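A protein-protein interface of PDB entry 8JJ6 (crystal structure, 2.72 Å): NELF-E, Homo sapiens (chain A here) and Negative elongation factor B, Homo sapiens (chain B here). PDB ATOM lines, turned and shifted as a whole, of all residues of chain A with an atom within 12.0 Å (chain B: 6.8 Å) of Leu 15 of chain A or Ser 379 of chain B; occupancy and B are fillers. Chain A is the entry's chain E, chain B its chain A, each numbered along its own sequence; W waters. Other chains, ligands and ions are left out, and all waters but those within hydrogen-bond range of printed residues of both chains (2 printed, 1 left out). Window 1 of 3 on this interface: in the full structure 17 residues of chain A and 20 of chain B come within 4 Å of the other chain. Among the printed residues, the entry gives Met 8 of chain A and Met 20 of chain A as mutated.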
ATOM      1  N   MET A   8     -25.748  25.954 -21.902  1.00  0.00           N
ATOM      2  CA  MET A   8     -26.069  25.155 -20.731  1.00  0.00           C
ATOM      3  C   MET A   8     -26.289  26.026 -19.507  1.00  0.00           C
ATOM      4  O   MET A   8     -25.695  27.095 -19.349  1.00  0.00           O
ATOM      5  CB  MET A   8     -24.970  24.137 -20.447  1.00  0.00           C
ATOM      6  CG  MET A   8     -25.342  22.759 -20.965  1.00  0.00           C
ATOM      7  SD  MET A   8     -23.908  21.728 -21.172  1.00  0.00           S
ATOM      8  CE  MET A   8     -23.185  21.773 -19.552  1.00  0.00           C
ATOM      9  N   SER A   9     -27.181  25.566 -18.648  1.00  0.00           N
ATOM     10  CA  SER A   9     -27.429  26.282 -17.417  1.00  0.00           C
ATOM     11  C   SER A   9     -26.356  25.923 -16.403  1.00  0.00           C
ATOM     12  O   SER A   9     -25.549  25.017 -16.605  1.00  0.00           O
ATOM     13  CB  SER A   9     -28.811  25.946 -16.861  1.00  0.00           C
ATOM     14  OG  SER A   9     -28.779  24.710 -16.166  1.00  0.00           O
ATOM     15  N   GLU A  10     -26.370  26.644 -15.288  1.00  0.00           N
ATOM     16  CA  GLU A  10     -25.446  26.330 -14.214  1.00  0.00           C
ATOM     17  C   GLU A  10     -25.619  24.895 -13.748  1.00  0.00           C
ATOM     18  O   GLU A  10     -24.646  24.139 -13.662  1.00  0.00           O
ATOM     19  CB  GLU A  10     -25.658  27.303 -13.069  1.00  0.00           C
ATOM     20  CG  GLU A  10     -24.530  28.289 -12.943  1.00  0.00           C
ATOM     21  CD  GLU A  10     -24.974  29.565 -12.297  1.00  0.00           C
ATOM     22  OE1 GLU A  10     -25.797  29.495 -11.349  1.00  0.00           O
ATOM     23  OE2 GLU A  10     -24.504  30.633 -12.744  1.00  0.00           O
ATOM     24  N   GLU A  11     -26.862  24.499 -13.455  1.00  0.00           N
ATOM     25  CA  GLU A  11     -27.124  23.159 -12.940  1.00  0.00           C
ATOM     26  C   GLU A  11     -26.705  22.090 -13.941  1.00  0.00           C
ATOM     27  O   GLU A  11     -26.233  21.014 -13.546  1.00  0.00           O
ATOM     28  CB  GLU A  11     -28.606  23.028 -12.587  1.00  0.00           C
ATOM     29  CG  GLU A  11     -29.110  23.991 -11.492  1.00  0.00           C
ATOM     30  CD  GLU A  11     -29.537  25.373 -12.023  1.00  0.00           C
ATOM     31  OE1 GLU A  11     -29.154  25.748 -13.161  1.00  0.00           O
ATOM     32  OE2 GLU A  11     -30.250  26.101 -11.284  1.00  0.00           O
ATOM     33  N   GLU A  12     -26.846  22.371 -15.240  1.00  0.00           N
ATOM     34  CA  GLU A  12     -26.379  21.425 -16.252  1.00  0.00           C
ATOM     35  C   GLU A  12     -24.860  21.243 -16.184  1.00  0.00           C
ATOM     36  O   GLU A  12     -24.365  20.111 -16.106  1.00  0.00           O
ATOM     37  CB  GLU A  12     -26.830  21.887 -17.637  1.00  0.00           C
ATOM     38  CG  GLU A  12     -28.189  21.331 -18.039  1.00  0.00           C
ATOM     39  CD  GLU A  12     -28.941  22.184 -19.063  1.00  0.00           C
ATOM     40  OE1 GLU A  12     -28.573  23.350 -19.325  1.00  0.00           O
ATOM     41  OE2 GLU A  12     -29.932  21.686 -19.603  1.00  0.00           O
ATOM     42  N   GLU A  13     -24.095  22.346 -16.197  1.00  0.00           N
ATOM     43  CA  GLU A  13     -22.636  22.227 -16.128  1.00  0.00           C
ATOM     44  C   GLU A  13     -22.179  21.552 -14.840  1.00  0.00           C
ATOM     45  O   GLU A  13     -21.208  20.792 -14.857  1.00  0.00           O
ATOM     46  CB  GLU A  13     -21.962  23.595 -16.263  1.00  0.00           C
ATOM     47  CG  GLU A  13     -22.359  24.367 -17.497  1.00  0.00           C
ATOM     48  CD  GLU A  13     -21.862  25.805 -17.497  1.00  0.00           C
ATOM     49  OE1 GLU A  13     -21.683  26.385 -16.393  1.00  0.00           O
ATOM     50  OE2 GLU A  13     -21.666  26.352 -18.612  1.00  0.00           O
ATOM     51  N   ALA A  14     -22.847  21.826 -13.716  1.00  0.00           N
ATOM     52  CA  ALA A  14     -22.551  21.079 -12.499  1.00  0.00           C
ATOM     53  C   ALA A  14     -22.785  19.579 -12.707  1.00  0.00           C
ATOM     54  O   ALA A  14     -21.957  18.747 -12.301  1.00  0.00           O
ATOM     55  CB  ALA A  14     -23.390  21.619 -11.344  1.00  0.00           C
ATOM     56  N   LEU A  15     -23.893  19.213 -13.364  1.00  0.00           N
ATOM     57  CA  LEU A  15     -24.159  17.805 -13.641  1.00  0.00           C
ATOM     58  C   LEU A  15     -23.041  17.194 -14.469  1.00  0.00           C
ATOM     59  O   LEU A  15     -22.542  16.104 -14.157  1.00  0.00           O
ATOM     60  CB  LEU A  15     -25.494  17.653 -14.370  1.00  0.00           C
ATOM     61  CG  LEU A  15     -26.378  16.464 -13.992  1.00  0.00           C
ATOM     62  CD1 LEU A  15     -27.252  16.076 -15.163  1.00  0.00           C
ATOM     63  CD2 LEU A  15     -25.583  15.265 -13.469  1.00  0.00           C
ATOM     64  N   GLN A  16     -22.635  17.882 -15.534  1.00  0.00           N
ATOM     65  CA  GLN A  16     -21.575  17.343 -16.371  1.00  0.00           C
ATOM     66  C   GLN A  16     -20.255  17.249 -15.612  1.00  0.00           C
ATOM     67  O   GLN A  16     -19.454  16.348 -15.876  1.00  0.00           O
ATOM     68  CB  GLN A  16     -21.438  18.197 -17.615  1.00  0.00           C
ATOM     69  CG  GLN A  16     -21.255  17.417 -18.890  1.00  0.00           C
ATOM     70  CD  GLN A  16     -21.941  18.088 -20.078  1.00  0.00           C
ATOM     71  OE1 GLN A  16     -23.019  18.676 -19.927  1.00  0.00           O
ATOM     72  NE2 GLN A  16     -21.276  18.069 -21.251  1.00  0.00           N
ATOM     73  N   LYS A  17     -20.025  18.134 -14.641  1.00  0.00           N
ATOM     74  CA  LYS A  17     -18.829  18.020 -13.805  1.00  0.00           C
ATOM     75  C   LYS A  17     -18.921  16.824 -12.864  1.00  0.00           C
ATOM     76  O   LYS A  17     -17.971  16.039 -12.752  1.00  0.00           O
ATOM     77  CB  LYS A  17     -18.599  19.316 -13.028  1.00  0.00           C
ATOM     78  CG  LYS A  17     -17.542  20.192 -13.686  1.00  0.00           C
ATOM     79  CD  LYS A  17     -17.850  21.687 -13.588  1.00  0.00           C
ATOM     80  CE  LYS A  17     -16.802  22.511 -14.352  1.00  0.00           C
ATOM     81  NZ  LYS A  17     -16.710  23.936 -13.915  1.00  0.00           N
ATOM     82  N   LYS A  18     -20.056  16.651 -12.192  1.00  0.00           N
ATOM     83  CA  LYS A  18     -20.217  15.451 -11.388  1.00  0.00           C
ATOM     84  C   LYS A  18     -20.091  14.192 -12.242  1.00  0.00           C
ATOM     85  O   LYS A  18     -19.589  13.171 -11.762  1.00  0.00           O
ATOM     86  CB  LYS A  18     -21.556  15.486 -10.659  1.00  0.00           C
ATOM     87  CG  LYS A  18     -21.561  16.367  -9.439  1.00  0.00           C
ATOM     88  CD  LYS A  18     -22.976  16.781  -9.114  1.00  0.00           C
ATOM     89  CE  LYS A  18     -23.024  17.974  -8.183  1.00  0.00           C
ATOM     90  NZ  LYS A  18     -23.165  17.542  -6.759  1.00  0.00           N
ATOM     91  N   PHE A  19     -20.536  14.242 -13.506  1.00  0.00           N
ATOM     92  CA  PHE A  19     -20.360  13.097 -14.404  1.00  0.00           C
ATOM     93  C   PHE A  19     -18.893  12.720 -14.528  1.00  0.00           C
ATOM     94  O   PHE A  19     -18.530  11.544 -14.409  1.00  0.00           O
ATOM     95  CB  PHE A  19     -20.912  13.411 -15.796  1.00  0.00           C
ATOM     96  CG  PHE A  19     -22.359  13.156 -15.940  1.00  0.00           C
ATOM     97  CD1 PHE A  19     -23.003  12.277 -15.097  1.00  0.00           C
ATOM     98  CD2 PHE A  19     -23.086  13.816 -16.918  1.00  0.00           C
ATOM     99  CE1 PHE A  19     -24.350  12.067 -15.229  1.00  0.00           C
ATOM    100  CE2 PHE A  19     -24.432  13.607 -17.063  1.00  0.00           C
ATOM    101  CZ  PHE A  19     -25.068  12.734 -16.222  1.00  0.00           C
ATOM    102  N   MET A  20     -18.039  13.722 -14.784  1.00  0.00           N
ATOM    103  CA  MET A  20     -16.626  13.466 -15.030  1.00  0.00           C
ATOM    104  C   MET A  20     -15.917  13.094 -13.742  1.00  0.00           C
ATOM    105  O   MET A  20     -15.055  12.210 -13.734  1.00  0.00           O
ATOM    106  CB  MET A  20     -15.981  14.689 -15.688  1.00  0.00           C
ATOM    107  CG  MET A  20     -16.499  14.938 -17.112  1.00  0.00           C
ATOM    108  SD  MET A  20     -15.894  16.430 -17.962  1.00  0.00           S
ATOM    109  CE  MET A  20     -16.796  17.768 -17.165  1.00  0.00           C
ATOM    110  N   LYS A  21     -16.291  13.733 -12.638  1.00  0.00           N
ATOM    111  CA  LYS A  21     -15.739  13.342 -11.352  1.00  0.00           C
ATOM    112  C   LYS A  21     -15.994  11.867 -11.085  1.00  0.00           C
ATOM    113  O   LYS A  21     -15.124  11.171 -10.556  1.00  0.00           O
ATOM    114  CB  LYS A  21     -16.328  14.217 -10.246  1.00  0.00           C
ATOM    115  CG  LYS A  21     -15.612  14.092  -8.916  1.00  0.00           C
ATOM    116  CD  LYS A  21     -16.246  14.993  -7.862  1.00  0.00           C
ATOM    117  CE  LYS A  21     -15.257  15.327  -6.758  1.00  0.00           C
ATOM    118  NZ  LYS A  21     -15.848  16.240  -5.731  1.00  0.00           N
ATOM    119  N   LEU A  22     -17.163  11.363 -11.491  1.00  0.00           N
ATOM    120  CA  LEU A  22     -17.521   9.966 -11.264  1.00  0.00           C
ATOM    121  C   LEU A  22     -16.825   9.023 -12.235  1.00  0.00           C
ATOM    122  O   LEU A  22     -16.584   7.857 -11.899  1.00  0.00           O
ATOM    123  CB  LEU A  22     -19.033   9.779 -11.385  1.00  0.00           C
ATOM    124  CG  LEU A  22     -19.590   8.401 -11.011  1.00  0.00           C
ATOM    125  CD1 LEU A  22     -19.071   7.957  -9.645  1.00  0.00           C
ATOM    126  CD2 LEU A  22     -21.093   8.401 -11.054  1.00  0.00           C
ATOM    127  N   LYS A  23     -16.530   9.490 -13.447  1.00  0.00           N
ATOM    128  CA  LYS A  23     -15.796   8.655 -14.386  1.00  0.00           C
ATOM    129  C   LYS A  23     -14.406   8.354 -13.844  1.00  0.00           C
ATOM    130  O   LYS A  23     -14.002   7.187 -13.754  1.00  0.00           O
ATOM    131  CB  LYS A  23     -15.724   9.348 -15.745  1.00  0.00           C
ATOM    132  CG  LYS A  23     -15.552   8.416 -16.917  1.00  0.00           C
ATOM    133  CD  LYS A  23     -15.971   9.119 -18.203  1.00  0.00           C
ATOM    134  CE  LYS A  23     -16.357   8.119 -19.305  1.00  0.00           C
ATOM    135  NZ  LYS A  23     -17.681   7.433 -19.095  1.00  0.00           N
ATOM    136  N   LYS A  24     -13.684   9.405 -13.430  1.00  0.00           N
ATOM    137  CA  LYS A  24     -12.353   9.246 -12.845  1.00  0.00           C
ATOM    138  C   LYS A  24     -12.372   8.272 -11.675  1.00  0.00           C
ATOM    139  O   LYS A  24     -11.557   7.345 -11.613  1.00  0.00           O
ATOM    140  CB  LYS A  24     -11.807  10.599 -12.380  1.00  0.00           C
ATOM    141  CG  LYS A  24     -11.496  11.602 -13.486  1.00  0.00           C
ATOM    142  CD  LYS A  24     -10.905  12.870 -12.881  1.00  0.00           C
ATOM    143  CE  LYS A  24     -11.158  14.089 -13.757  1.00  0.00           C
ATOM    144  NZ  LYS A  24     -10.922  15.367 -13.009  1.00  0.00           N
ATOM    145  N   VAL B 326     -28.255   8.951 -16.359  1.00  0.00           N
ATOM    146  CA  VAL B 326     -27.020   9.117 -15.611  1.00  0.00           C
ATOM    147  C   VAL B 326     -25.959   8.167 -16.149  1.00  0.00           C
ATOM    148  O   VAL B 326     -24.836   8.575 -16.466  1.00  0.00           O
ATOM    149  CB  VAL B 326     -27.276   8.904 -14.111  1.00  0.00           C
ATOM    150  CG1 VAL B 326     -25.962   8.873 -13.361  1.00  0.00           C
ATOM    151  CG2 VAL B 326     -28.181  10.006 -13.561  1.00  0.00           C
ATOM    152  N   THR B 330     -26.128  11.783 -20.109  1.00  0.00           N
ATOM    153  CA  THR B 330     -26.881  12.651 -21.013  1.00  0.00           C
ATOM    154  C   THR B 330     -27.733  13.642 -20.225  1.00  0.00           C
ATOM    155  O   THR B 330     -28.247  13.315 -19.159  1.00  0.00           O
ATOM    156  CB  THR B 330     -27.783  11.807 -21.925  1.00  0.00           C
ATOM    157  OG1 THR B 330     -26.975  10.891 -22.677  1.00  0.00           O
ATOM    158  CG2 THR B 330     -28.633  12.672 -22.862  1.00  0.00           C
ATOM    159  N   LEU B 331     -27.889  14.861 -20.746  1.00  0.00           N
ATOM    160  CA  LEU B 331     -28.748  15.800 -20.023  1.00  0.00           C
ATOM    161  C   LEU B 331     -30.229  15.558 -20.360  1.00  0.00           C
ATOM    162  O   LEU B 331     -30.559  15.077 -21.449  1.00  0.00           O
ATOM    163  CB  LEU B 331     -28.376  17.245 -20.362  1.00  0.00           C
ATOM    164  CG  LEU B 331     -26.891  17.601 -20.214  1.00  0.00           C
ATOM    165  CD1 LEU B 331     -26.520  18.992 -20.767  1.00  0.00           C
ATOM    166  CD2 LEU B 331     -26.536  17.483 -18.757  1.00  0.00           C
ATOM    167  N   PRO B 332     -31.141  15.875 -19.438  1.00  0.00           N
ATOM    168  CA  PRO B 332     -32.574  15.759 -19.761  1.00  0.00           C
ATOM    169  C   PRO B 332     -32.991  16.405 -21.082  1.00  0.00           C
ATOM    170  O   PRO B 332     -33.828  15.851 -21.807  1.00  0.00           O
ATOM    171  CB  PRO B 332     -33.234  16.438 -18.557  1.00  0.00           C
ATOM    172  CG  PRO B 332     -32.326  16.125 -17.432  1.00  0.00           C
ATOM    173  CD  PRO B 332     -30.922  16.120 -18.001  1.00  0.00           C
ATOM    174  N   LEU B 374     -34.669  18.914 -13.229  1.00  0.00           N
ATOM    175  CA  LEU B 374     -34.243  17.551 -13.508  1.00  0.00           C
ATOM    176  C   LEU B 374     -32.727  17.411 -13.433  1.00  0.00           C
ATOM    177  O   LEU B 374     -32.255  16.368 -12.945  1.00  0.00           O
ATOM    178  CB  LEU B 374     -34.799  17.113 -14.870  1.00  0.00           C
ATOM    179  CG  LEU B 374     -36.317  16.879 -14.893  1.00  0.00           C
ATOM    180  CD1 LEU B 374     -36.775  16.378 -16.251  1.00  0.00           C
ATOM    181  CD2 LEU B 374     -36.816  15.952 -13.760  1.00  0.00           C
ATOM    182  N   PRO B 375     -31.921  18.374 -13.893  1.00  0.00           N
ATOM    183  CA  PRO B 375     -30.481  18.250 -13.664  1.00  0.00           C
ATOM    184  C   PRO B 375     -30.097  18.169 -12.196  1.00  0.00           C
ATOM    185  O   PRO B 375     -29.181  17.406 -11.849  1.00  0.00           O
ATOM    186  CB  PRO B 375     -29.934  19.500 -14.359  1.00  0.00           C
ATOM    187  CG  PRO B 375     -30.817  19.629 -15.510  1.00  0.00           C
ATOM    188  CD  PRO B 375     -32.187  19.361 -14.960  1.00  0.00           C
ATOM    189  N   MET B 376     -30.771  18.903 -11.312  1.00  0.00           N
ATOM    190  CA  MET B 376     -30.427  18.779  -9.900  1.00  0.00           C
ATOM    191  C   MET B 376     -30.832  17.421  -9.361  1.00  0.00           C
ATOM    192  O   MET B 376     -30.102  16.824  -8.563  1.00  0.00           O
ATOM    193  CB  MET B 376     -31.062  19.900  -9.095  1.00  0.00           C
ATOM    194  CG  MET B 376     -30.278  21.198  -9.201  1.00  0.00           C
ATOM    195  SD  MET B 376     -31.401  22.580  -9.072  1.00  0.00           S
ATOM    196  CE  MET B 376     -31.484  22.654  -7.330  1.00  0.00           C
ATOM    197  N   LEU B 377     -31.969  16.898  -9.816  1.00  0.00           N
ATOM    198  CA  LEU B 377     -32.354  15.542  -9.446  1.00  0.00           C
ATOM    199  C   LEU B 377     -31.253  14.546  -9.794  1.00  0.00           C
ATOM    200  O   LEU B 377     -30.818  13.781  -8.933  1.00  0.00           O
ATOM    201  CB  LEU B 377     -33.670  15.164 -10.123  1.00  0.00           C
ATOM    202  CG  LEU B 377     -34.881  15.193  -9.190  1.00  0.00           C
ATOM    203  CD1 LEU B 377     -35.991  14.249  -9.668  1.00  0.00           C
ATOM    204  CD2 LEU B 377     -34.470  14.876  -7.768  1.00  0.00           C
ATOM    205  N   MET B 378     -30.783  14.536 -11.053  1.00  0.00           N
ATOM    206  CA  MET B 378     -29.729  13.592 -11.433  1.00  0.00           C
ATOM    207  C   MET B 378     -28.426  13.815 -10.668  1.00  0.00           C
ATOM    208  O   MET B 378     -27.691  12.846 -10.418  1.00  0.00           O
ATOM    209  CB  MET B 378     -29.440  13.625 -12.935  1.00  0.00           C
ATOM    210  CG  MET B 378     -30.580  13.097 -13.838  1.00  0.00           C
ATOM    211  SD  MET B 378     -30.495  13.554 -15.594  1.00  0.00           S
ATOM    212  CE  MET B 378     -29.219  12.342 -16.082  1.00  0.00           C
ATOM    213  N   SER B 379     -28.138  15.062 -10.273  1.00  0.00           N
ATOM    214  CA  SER B 379     -26.963  15.329  -9.447  1.00  0.00           C
ATOM    215  C   SER B 379     -27.018  14.551  -8.136  1.00  0.00           C
ATOM    216  O   SER B 379     -26.019  13.943  -7.723  1.00  0.00           O
ATOM    217  CB  SER B 379     -26.839  16.819  -9.179  1.00  0.00           C
ATOM    218  OG  SER B 379     -26.444  17.490 -10.362  1.00  0.00           O
ATOM    219  N   PHE B 380     -28.183  14.535  -7.472  1.00  0.00           N
ATOM    220  CA  PHE B 380     -28.315  13.729  -6.263  1.00  0.00           C
ATOM    221  C   PHE B 380     -27.963  12.270  -6.536  1.00  0.00           C
ATOM    222  O   PHE B 380     -27.317  11.619  -5.704  1.00  0.00           O
ATOM    223  CB  PHE B 380     -29.730  13.832  -5.680  1.00  0.00           C
ATOM    224  CG  PHE B 380     -30.148  15.231  -5.321  1.00  0.00           C
ATOM    225  CD1 PHE B 380     -29.208  16.214  -5.081  1.00  0.00           C
ATOM    226  CD2 PHE B 380     -31.496  15.560  -5.245  1.00  0.00           C
ATOM    227  CE1 PHE B 380     -29.588  17.498  -4.769  1.00  0.00           C
ATOM    228  CE2 PHE B 380     -31.893  16.852  -4.917  1.00  0.00           C
ATOM    229  CZ  PHE B 380     -30.926  17.822  -4.680  1.00  0.00           C
ATOM    230  N   LEU B 381     -28.369  11.740  -7.698  1.00  0.00           N
ATOM    231  CA  LEU B 381     -27.958  10.391  -8.079  1.00  0.00           C
ATOM    232  C   LEU B 381     -26.456  10.294  -8.237  1.00  0.00           C
ATOM    233  O   LEU B 381     -25.823   9.387  -7.690  1.00  0.00           O
ATOM    234  CB  LEU B 381     -28.606   9.971  -9.385  1.00  0.00           C
ATOM    235  CG  LEU B 381     -29.802   9.085  -9.133  1.00  0.00           C
ATOM    236  CD1 LEU B 381     -30.829  10.042  -8.761  1.00  0.00           C
ATOM    237  CD2 LEU B 381     -30.188   8.334 -10.377  1.00  0.00           C
ATOM    238  N   VAL B 382     -25.875  11.192  -9.031  1.00  0.00           N
ATOM    239  CA  VAL B 382     -24.449  11.102  -9.297  1.00  0.00           C
ATOM    240  C   VAL B 382     -23.672  11.302  -8.007  1.00  0.00           C
ATOM    241  O   VAL B 382     -22.644  10.646  -7.775  1.00  0.00           O
ATOM    242  CB  VAL B 382     -24.045  12.112 -10.381  1.00  0.00           C
ATOM    243  CG1 VAL B 382     -22.534  12.089 -10.592  1.00  0.00           C
ATOM    244  CG2 VAL B 382     -24.765  11.782 -11.660  1.00  0.00           C
ATOM    245  N   ASP B 383     -24.163  12.191  -7.138  1.00  0.00           N
ATOM    246  CA  ASP B 383     -23.576  12.333  -5.814  1.00  0.00           C
ATOM    247  C   ASP B 383     -23.537  10.988  -5.114  1.00  0.00           C
ATOM    248  O   ASP B 383     -22.486  10.536  -4.652  1.00  0.00           O
ATOM    249  CB  ASP B 383     -24.389  13.329  -4.988  1.00  0.00           C
ATOM    250  CG  ASP B 383     -24.080  14.772  -5.331  1.00  0.00           C
ATOM    251  OD1 ASP B 383     -23.074  15.014  -6.062  1.00  0.00           O
ATOM    252  OD2 ASP B 383     -24.848  15.656  -4.861  1.00  0.00           O
ATOM    253  N   ASP B 384     -24.687  10.324  -5.051  1.00  0.00           N
ATOM    254  CA  ASP B 384     -24.794   9.072  -4.324  1.00  0.00           C
ATOM    255  C   ASP B 384     -23.967   7.976  -4.977  1.00  0.00           C
ATOM    256  O   ASP B 384     -23.442   7.100  -4.277  1.00  0.00           O
ATOM    257  CB  ASP B 384     -26.259   8.667  -4.236  1.00  0.00           C
ATOM    258  CG  ASP B 384     -26.476   7.517  -3.314  1.00  0.00           C
ATOM    259  OD1 ASP B 384     -26.503   6.360  -3.793  1.00  0.00           O
ATOM    260  OD2 ASP B 384     -26.603   7.772  -2.099  1.00  0.00           O
ATOM    261  N   TYR B 385     -23.834   8.001  -6.307  1.00  0.00           N
ATOM    262  CA  TYR B 385     -22.928   7.059  -6.955  1.00  0.00           C
ATOM    263  C   TYR B 385     -21.484   7.352  -6.573  1.00  0.00           C
ATOM    264  O   TYR B 385     -20.692   6.429  -6.347  1.00  0.00           O
ATOM    265  CB  TYR B 385     -23.086   7.113  -8.476  1.00  0.00           C
ATOM    266  CG  TYR B 385     -24.339   6.459  -9.025  1.00  0.00           C
ATOM    267  CD1 TYR B 385     -24.881   5.317  -8.433  1.00  0.00           C
ATOM    268  CD2 TYR B 385     -24.976   6.983 -10.144  1.00  0.00           C
ATOM    269  CE1 TYR B 385     -26.036   4.722  -8.947  1.00  0.00           C
ATOM    270  CE2 TYR B 385     -26.123   6.404 -10.654  1.00  0.00           C
ATOM    271  CZ  TYR B 385     -26.647   5.274 -10.059  1.00  0.00           C
ATOM    272  OH  TYR B 385     -27.785   4.709 -10.586  1.00  0.00           O
ATOM    273  N   TYR B 428     -38.781  10.308  -6.760  1.00  0.00           N
ATOM    274  CA  TYR B 428     -37.377  10.060  -6.503  1.00  0.00           C
ATOM    275  C   TYR B 428     -37.132   9.780  -5.011  1.00  0.00           C
ATOM    276  O   TYR B 428     -36.283   8.951  -4.665  1.00  0.00           O
ATOM    277  CB  TYR B 428     -36.551  11.232  -7.014  1.00  0.00           C
ATOM    278  CG  TYR B 428     -35.163  11.133  -6.498  1.00  0.00           C
ATOM    279  CD1 TYR B 428     -34.217  10.430  -7.182  1.00  0.00           C
ATOM    280  CD2 TYR B 428     -34.811  11.698  -5.281  1.00  0.00           C
ATOM    281  CE1 TYR B 428     -32.956  10.291  -6.670  1.00  0.00           C
ATOM    282  CE2 TYR B 428     -33.545  11.567  -4.777  1.00  0.00           C
ATOM    283  CZ  TYR B 428     -32.608  10.874  -5.480  1.00  0.00           C
ATOM    284  OH  TYR B 428     -31.321  10.752  -4.979  1.00  0.00           O
ATOM    285  N   ARG B 443     -31.268  13.379   3.482  1.00  0.00           N
ATOM    286  CA  ARG B 443     -30.892  14.585   2.754  1.00  0.00           C
ATOM    287  C   ARG B 443     -32.113  15.249   2.133  1.00  0.00           C
ATOM    288  O   ARG B 443     -32.241  16.476   2.182  1.00  0.00           O
ATOM    289  CB  ARG B 443     -29.845  14.263   1.690  1.00  0.00           C
ATOM    290  CG  ARG B 443     -29.343  15.454   0.901  1.00  0.00           C
ATOM    291  CD  ARG B 443     -28.642  15.015  -0.368  1.00  0.00           C
ATOM    292  NE  ARG B 443     -28.046  16.147  -1.080  1.00  0.00           N
ATOM    293  CZ  ARG B 443     -27.121  16.047  -2.040  1.00  0.00           C
ATOM    294  NH1 ARG B 443     -26.667  14.863  -2.416  1.00  0.00           N
ATOM    295  NH2 ARG B 443     -26.651  17.129  -2.637  1.00  0.00           N
HETATM  296  O   HOH W   1     -26.976  20.457 -10.751  1.00  0.00           O
HETATM  297  O   HOH W   2     -26.003  17.719  -5.500  1.00  0.00           O
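Water W2 lies within hydrogen-bond range of the side-chain carboxylate of Asp 383 of chain B (2.4 Å), the guanidinium group of Arg 443 of chain B (3.0 Å) and the side-chain amino group of Lys 18 of chain A (3.1 Å).
Water W1 lies within hydrogen-bond range of O of Glu 11 of chain A (2.9 Å) and OG of Ser 379 of chain B (3.0 Å).
Of the 18 printed residues of chain B, 10 touch a printed residue of chain A.
Hydrophobic or aromatic side chains of chain B within 4 Å of the printed part of chain A: Leu 331, Met 376, Met 378, Val 382 and Tyr 385.
Printed residues of chain A that touch a printed residue of chain B: Met 8, Glu 11, Glu 12, Leu 15, Gln 16, Lys 18, Phe 19 and Leu 22.
Hydrophobic or aromatic side chains of chain A that line the printed part of chain B: Met 8, Leu 15, Phe 19 and Leu 22.
Among the printed residues, 16 pairs touch across the chains.
Among the printed residues, Asp or Glu carboxylates within 4 Å of a Lys or Arg side-chain nitrogen of the other chain: Lys 18 of chain A with Asp 383 of chain B.
Ser 379 of chain B touches just these residues of chain A: Leu 15 (3.8 Å) and Lys 18 (3.8 Å).
Of chain A, only Leu 15 (3.7 Å) comes within 4 Å of Pro 375 of chain B.
Printed residues of chain A within 4 Å of Met 376 of chain B: Glu 11 (3.6 Å).
No residue of chain A comes within 4 Å of Phe 380 of chain B.
No residue of chain A comes within 4 Å of Leu 381 of chain B.
Of chain A, only Lys 18 (2.6 Å) comes within 4 Å of Asp 383 of chain B.
Of the printed residues of chain B, Met 8 of chain A touches Leu 331.
Of the printed residues of chain B, Leu 22 of chain A touches Val 382 (3.99 Å) and Tyr 385 (3.5 Å).
Of the printed residues of chain B, Lys 18 of chain A touches Ser 379, Val 382 and Asp 383.
Of the printed residues of chain B, Gln 16 of chain A touches Leu 331.
Pro 332 of chain B touches none of the printed residues of chain A.
The nearest printed residue of chain B that does not touch Gln 16 of chain A is Ser 379 of chain B (6.4 Å).
Met 8 of chain A touches Leu 331 of chain B (SD to CD1, 3.8 Å).
CG of Glu 11 of chain A touches SD of Met 376 of chain B (3.6 Å).
CD1 of Leu 331 of chain B touches CG of Glu 12 of chain A (3.96 Å).
Leu 15 of chain A touches Ser 379 of chain B (CG to OG, 3.8 Å).
OG of Ser 379 of chain B touches CD of Lys 18 of chain A, at 3.8 Å.
Lys 18 of chain A touches Val 382 of chain B.
Phe 19 of chain A touches Val 326 of chain B.
Phe 19 of chain A touches Val 382 of chain B (CE1 to CG2, 3.6 Å).
Val 382 of chain B touches Leu 22 of chain A.
CD2 of Leu 22 of chain A touches CB of Tyr 385 of chain B, at 3.5 Å.
O of Pro 375 of chain B is in hydrogen-bond range of OG of Ser 379 of chain B (3.1 Å).
The side-chain carboxylate of Asp 383 of chain B lies within salt-bridge range of the guanidinium group of Arg 443 of chain B, at 3.1 Å.
The side-chain sulfur (SD) of Met 8 of chain A sits close to the side-chain amide oxygen (OE1) of Gln 16 of chain A.
The side-chain hydroxyl (OG) of Ser 9 of chain A lies within hydrogen-bond range of the side-chain carboxylate (OE1) of Glu 11 of chain A.
N of Ser 9 of chain A is in hydrogen-bond range of OE1 of Glu 12 of chain A (2.7 Å).
OD1 of Asp 383 of chain B lies within salt-bridge range of NZ of Lys 18 of chain A (2.6 Å).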
